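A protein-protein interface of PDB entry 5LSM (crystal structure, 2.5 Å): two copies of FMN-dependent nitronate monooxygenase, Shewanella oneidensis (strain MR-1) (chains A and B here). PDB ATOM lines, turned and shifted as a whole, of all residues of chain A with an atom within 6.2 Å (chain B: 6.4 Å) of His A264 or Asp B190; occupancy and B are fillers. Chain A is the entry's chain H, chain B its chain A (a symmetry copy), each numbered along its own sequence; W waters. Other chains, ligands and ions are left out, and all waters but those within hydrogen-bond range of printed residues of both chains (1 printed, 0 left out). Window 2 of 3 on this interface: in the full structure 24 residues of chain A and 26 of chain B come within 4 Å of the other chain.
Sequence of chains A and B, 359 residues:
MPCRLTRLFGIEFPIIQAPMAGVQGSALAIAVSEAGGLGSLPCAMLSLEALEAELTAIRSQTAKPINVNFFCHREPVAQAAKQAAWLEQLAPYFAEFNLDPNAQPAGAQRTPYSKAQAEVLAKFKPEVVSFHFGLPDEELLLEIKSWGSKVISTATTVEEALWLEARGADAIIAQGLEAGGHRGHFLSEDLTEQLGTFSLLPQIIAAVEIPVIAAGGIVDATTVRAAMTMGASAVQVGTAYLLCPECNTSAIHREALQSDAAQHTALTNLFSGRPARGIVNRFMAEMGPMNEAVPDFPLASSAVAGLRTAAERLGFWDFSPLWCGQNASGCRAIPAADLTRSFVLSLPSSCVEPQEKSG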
ATOM      1  N   ASP A 260      26.677 -15.111 -27.542  1.00  0.00           N
ATOM      2  CA  ASP A 260      26.358 -15.686 -26.242  1.00  0.00           C
ATOM      3  C   ASP A 260      25.253 -16.732 -26.357  1.00  0.00           C
ATOM      4  O   ASP A 260      25.095 -17.574 -25.480  1.00  0.00           O
ATOM      5  CB  ASP A 260      25.932 -14.585 -25.269  1.00  0.00           C
ATOM      6  CG  ASP A 260      27.003 -13.527 -25.078  1.00  0.00           C
ATOM      7  OD1 ASP A 260      27.633 -13.501 -23.999  1.00  0.00           O
ATOM      8  OD2 ASP A 260      27.218 -12.720 -26.013  1.00  0.00           O
ATOM      9  N   ALA A 261      24.484 -16.670 -27.437  1.00  0.00           N
ATOM     10  CA  ALA A 261      23.553 -17.740 -27.780  1.00  0.00           C
ATOM     11  C   ALA A 261      24.225 -19.128 -27.821  1.00  0.00           C
ATOM     12  O   ALA A 261      23.615 -20.122 -27.444  1.00  0.00           O
ATOM     13  CB  ALA A 261      22.872 -17.438 -29.115  1.00  0.00           C
ATOM     14  N   ALA A 262      25.478 -19.187 -28.267  1.00  0.00           N
ATOM     15  CA  ALA A 262      26.212 -20.451 -28.361  1.00  0.00           C
ATOM     16  C   ALA A 262      26.218 -21.248 -27.060  1.00  0.00           C
ATOM     17  O   ALA A 262      26.279 -22.485 -27.076  1.00  0.00           O
ATOM     18  CB  ALA A 262      27.641 -20.192 -28.802  1.00  0.00           C
ATOM     19  N   GLN A 263      26.212 -20.549 -25.933  1.00  0.00           N
ATOM     20  CA  GLN A 263      26.304 -21.222 -24.642  1.00  0.00           C
ATOM     21  C   GLN A 263      25.096 -22.113 -24.363  1.00  0.00           C
ATOM     22  O   GLN A 263      25.226 -23.094 -23.620  1.00  0.00           O
ATOM     23  CB  GLN A 263      26.515 -20.222 -23.509  1.00  0.00           C
ATOM     24  CG  GLN A 263      27.870 -19.526 -23.545  1.00  0.00           C
ATOM     25  CD  GLN A 263      27.905 -18.275 -22.671  1.00  0.00           C
ATOM     26  OE1 GLN A 263      28.296 -17.196 -23.134  1.00  0.00           O
ATOM     27  NE2 GLN A 263      27.466 -18.406 -21.407  1.00  0.00           N
ATOM     28  N   HIS A 264      23.962 -21.821 -25.014  1.00  0.00           N
ATOM     29  CA  HIS A 264      22.731 -22.590 -24.839  1.00  0.00           C
ATOM     30  C   HIS A 264      22.388 -23.455 -26.067  1.00  0.00           C
ATOM     31  O   HIS A 264      22.085 -22.937 -27.161  1.00  0.00           O
ATOM     32  CB  HIS A 264      21.561 -21.659 -24.515  1.00  0.00           C
ATOM     33  CG  HIS A 264      20.274 -22.371 -24.210  1.00  0.00           C
ATOM     34  ND1 HIS A 264      19.059 -21.721 -24.152  1.00  0.00           N
ATOM     35  CD2 HIS A 264      20.014 -23.672 -23.934  1.00  0.00           C
ATOM     36  CE1 HIS A 264      18.104 -22.590 -23.869  1.00  0.00           C
ATOM     37  NE2 HIS A 264      18.659 -23.779 -23.717  1.00  0.00           N
ATOM     38  N   THR A 265      22.386 -24.771 -25.852  1.00  0.00           N
ATOM     39  CA  THR A 265      22.113 -25.748 -26.911  1.00  0.00           C
ATOM     40  C   THR A 265      21.085 -26.716 -26.396  1.00  0.00           C
ATOM     41  O   THR A 265      20.865 -26.808 -25.192  1.00  0.00           O
ATOM     42  CB  THR A 265      23.375 -26.569 -27.299  1.00  0.00           C
ATOM     43  OG1 THR A 265      23.842 -27.328 -26.169  1.00  0.00           O
ATOM     44  CG2 THR A 265      24.489 -25.663 -27.796  1.00  0.00           C
ATOM     45  N   ALA A 266      20.502 -27.488 -27.294  1.00  0.00           N
ATOM     46  CA  ALA A 266      19.537 -28.500 -26.895  1.00  0.00           C
ATOM     47  C   ALA A 266      19.374 -29.562 -27.967  1.00  0.00           C
ATOM     48  O   ALA A 266      19.658 -29.334 -29.135  1.00  0.00           O
ATOM     49  CB  ALA A 266      18.192 -27.859 -26.583  1.00  0.00           C
ATOM     50  N   GLY A 278      22.003 -28.654 -31.178  1.00  0.00           N
ATOM     51  CA  GLY A 278      22.331 -27.377 -31.797  1.00  0.00           C
ATOM     52  C   GLY A 278      22.009 -26.216 -30.898  1.00  0.00           C
ATOM     53  O   GLY A 278      21.337 -26.367 -29.887  1.00  0.00           O
ATOM     54  N   ILE A 279      22.526 -25.052 -31.263  1.00  0.00           N
ATOM     55  CA  ILE A 279      22.270 -23.825 -30.536  1.00  0.00           C
ATOM     56  C   ILE A 279      20.775 -23.496 -30.620  1.00  0.00           C
ATOM     57  O   ILE A 279      20.189 -23.536 -31.685  1.00  0.00           O
ATOM     58  CB  ILE A 279      23.094 -22.664 -31.132  1.00  0.00           C
ATOM     59  CG1 ILE A 279      24.595 -22.899 -30.880  1.00  0.00           C
ATOM     60  CG2 ILE A 279      22.622 -21.324 -30.559  1.00  0.00           C
ATOM     61  CD1 ILE A 279      25.520 -21.996 -31.674  1.00  0.00           C
ATOM     62  N   VAL A 280      20.181 -23.117 -29.500  1.00  0.00           N
ATOM     63  CA  VAL A 280      18.758 -22.864 -29.459  1.00  0.00           C
ATOM     64  C   VAL A 280      18.426 -21.608 -30.267  1.00  0.00           C
ATOM     65  O   VAL A 280      19.019 -20.563 -30.048  1.00  0.00           O
ATOM     66  CB  VAL A 280      18.274 -22.751 -27.999  1.00  0.00           C
ATOM     67  CG1 VAL A 280      16.802 -22.364 -27.932  1.00  0.00           C
ATOM     68  CG2 VAL A 280      18.502 -24.078 -27.284  1.00  0.00           C
ATOM     69  N   HIS B 185      19.717 -26.182  -9.422  1.00  0.00           N
ATOM     70  CA  HIS B 185      19.486 -24.963 -10.221  1.00  0.00           C
ATOM     71  C   HIS B 185      18.516 -23.986  -9.573  1.00  0.00           C
ATOM     72  O   HIS B 185      17.720 -24.353  -8.733  1.00  0.00           O
ATOM     73  CB  HIS B 185      18.967 -25.318 -11.612  1.00  0.00           C
ATOM     74  CG  HIS B 185      17.586 -25.883 -11.614  1.00  0.00           C
ATOM     75  ND1 HIS B 185      17.336 -27.231 -11.531  1.00  0.00           N
ATOM     76  CD2 HIS B 185      16.376 -25.283 -11.670  1.00  0.00           C
ATOM     77  CE1 HIS B 185      16.036 -27.445 -11.584  1.00  0.00           C
ATOM     78  NE2 HIS B 185      15.428 -26.277 -11.633  1.00  0.00           N
ATOM     79  N   SER B 188      16.876 -20.700 -13.446  1.00  0.00           N
ATOM     80  CA  SER B 188      16.004 -21.069 -14.563  1.00  0.00           C
ATOM     81  C   SER B 188      15.410 -22.459 -14.416  1.00  0.00           C
ATOM     82  O   SER B 188      16.081 -23.383 -13.969  1.00  0.00           O
ATOM     83  CB  SER B 188      16.786 -20.986 -15.872  1.00  0.00           C
ATOM     84  OG  SER B 188      16.057 -21.540 -16.955  1.00  0.00           O
ATOM     85  N   GLU B 189      14.173 -22.625 -14.863  1.00  0.00           N
ATOM     86  CA  GLU B 189      13.521 -23.939 -14.847  1.00  0.00           C
ATOM     87  C   GLU B 189      13.878 -24.785 -16.080  1.00  0.00           C
ATOM     88  O   GLU B 189      13.652 -25.982 -16.105  1.00  0.00           O
ATOM     89  CB  GLU B 189      12.006 -23.770 -14.748  1.00  0.00           C
ATOM     90  CG  GLU B 189      11.566 -22.906 -13.576  1.00  0.00           C
ATOM     91  CD  GLU B 189      10.353 -23.455 -12.840  1.00  0.00           C
ATOM     92  OE1 GLU B 189      10.119 -23.017 -11.692  1.00  0.00           O
ATOM     93  OE2 GLU B 189       9.627 -24.308 -13.407  1.00  0.00           O
ATOM     94  N   ASP B 190      14.459 -24.153 -17.087  1.00  0.00           N
ATOM     95  CA  ASP B 190      14.800 -24.827 -18.340  1.00  0.00           C
ATOM     96  C   ASP B 190      15.994 -25.780 -18.163  1.00  0.00           C
ATOM     97  O   ASP B 190      17.134 -25.345 -18.033  1.00  0.00           O
ATOM     98  CB  ASP B 190      15.115 -23.759 -19.389  1.00  0.00           C
ATOM     99  CG  ASP B 190      15.321 -24.328 -20.776  1.00  0.00           C
ATOM    100  OD1 ASP B 190      15.423 -25.577 -20.950  1.00  0.00           O
ATOM    101  OD2 ASP B 190      15.410 -23.497 -21.702  1.00  0.00           O
ATOM    102  N   LEU B 191      15.724 -27.079 -18.204  1.00  0.00           N
ATOM    103  CA  LEU B 191      16.761 -28.098 -18.047  1.00  0.00           C
ATOM    104  C   LEU B 191      17.772 -28.186 -19.206  1.00  0.00           C
ATOM    105  O   LEU B 191      18.894 -28.640 -19.003  1.00  0.00           O
ATOM    106  CB  LEU B 191      16.133 -29.473 -17.794  1.00  0.00           C
ATOM    107  CG  LEU B 191      15.352 -29.651 -16.477  1.00  0.00           C
ATOM    108  CD1 LEU B 191      14.823 -31.079 -16.377  1.00  0.00           C
ATOM    109  CD2 LEU B 191      16.198 -29.318 -15.258  1.00  0.00           C
ATOM    110  N   THR B 192      17.413 -27.701 -20.392  1.00  0.00           N
ATOM    111  CA  THR B 192      18.355 -27.693 -21.519  1.00  0.00           C
ATOM    112  C   THR B 192      19.490 -26.668 -21.352  1.00  0.00           C
ATOM    113  O   THR B 192      20.407 -26.607 -22.171  1.00  0.00           O
ATOM    114  CB  THR B 192      17.639 -27.398 -22.860  1.00  0.00           C
ATOM    115  OG1 THR B 192      17.199 -26.028 -22.894  1.00  0.00           O
ATOM    116  CG2 THR B 192      16.444 -28.360 -23.069  1.00  0.00           C
ATOM    117  N   GLU B 193      19.413 -25.830 -20.323  1.00  0.00           N
ATOM    118  CA  GLU B 193      20.514 -24.918 -20.011  1.00  0.00           C
ATOM    119  C   GLU B 193      21.649 -25.604 -19.247  1.00  0.00           C
ATOM    120  O   GLU B 193      22.789 -25.120 -19.240  1.00  0.00           O
ATOM    121  CB  GLU B 193      19.999 -23.702 -19.251  1.00  0.00           C
ATOM    122  CG  GLU B 193      19.001 -22.922 -20.075  1.00  0.00           C
ATOM    123  CD  GLU B 193      19.066 -21.435 -19.858  1.00  0.00           C
ATOM    124  OE1 GLU B 193      19.134 -21.000 -18.686  1.00  0.00           O
ATOM    125  OE2 GLU B 193      18.968 -20.702 -20.865  1.00  0.00           O
ATOM    126  N   GLN B 194      21.354 -26.768 -18.684  1.00  0.00           N
ATOM    127  CA  GLN B 194      22.301 -27.477 -17.844  1.00  0.00           C
ATOM    128  C   GLN B 194      23.206 -28.399 -18.658  1.00  0.00           C
ATOM    129  O   GLN B 194      22.874 -28.795 -19.772  1.00  0.00           O
ATOM    130  CB  GLN B 194      21.560 -28.257 -16.770  1.00  0.00           C
ATOM    131  CG  GLN B 194      20.846 -27.344 -15.783  1.00  0.00           C
ATOM    132  CD  GLN B 194      20.206 -28.107 -14.641  1.00  0.00           C
ATOM    133  OE1 GLN B 194      20.664 -29.188 -14.254  1.00  0.00           O
ATOM    134  NE2 GLN B 194      19.125 -27.561 -14.108  1.00  0.00           N
HETATM  135  O   HOH W   1      23.041 -25.265 -22.736  1.00  0.00           O
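A ring nitrogen (NE2) of His A264 lies within hydrogen-bond range of the side-chain hydroxyl (OG1) of Thr B192 (2.8 Å). A ring nitrogen (ND1) of His A264 lies within hydrogen-bond range of the side-chain carboxylate of Glu B193. O of Thr B192 sits close to O of Thr A265 (3.1 Å).
The backbone carbonyl oxygen of His A264 is in hydrogen-bond range of the backbone NH of Val A280 (3.0 Å). N of Ala A266 sits at hydrogen-bond distance from O of Gly A278, at 2.9 Å. The backbone NH (N) of Asp B190 lies within hydrogen-bond range of the side-chain hydroxyl (OG) of Ser B188 (3.1 Å). OG1 of Thr B192 sits at hydrogen-bond distance from OD1 of Asp B190 (2.7 Å).
His A264 touches Asp B190. Ala A266 touches Thr B192.
Of the printed residues of chain B, Thr A265 touches Thr B192. Of the printed residues of chain A, Thr B192 touches His A264 (2.8 Å), Thr A265 (3.1 Å) and Ala A266 (3.8 Å). Printed residues of chain B within 4 Å of Ala A266: Thr B192 (3.8 Å). Of the printed residues of chain A, Glu B193 touches His A264. The nearest printed residue of chain A that does not touch Asp B190 is Val A280 (6.4 Å).
Of the 8 printed residues of chain B, 3 touch a printed residue of chain A. Among the printed residues, 5 pairs touch across the chains. Among the printed residues, no Asp or Glu carboxylate lies within 4 Å of a Lys or Arg side-chain nitrogen of the other chain.
No position is printed for both chains. Of the 5 pairs that touch across the chains among the printed residues, none has its exchanged pair printed and touching as well.
Water W1 lies within hydrogen-bond range of O of Thr B192 (3.0 Å), O of Gln A263 (3.2 Å) and N of Thr A265 (3.2 Å).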
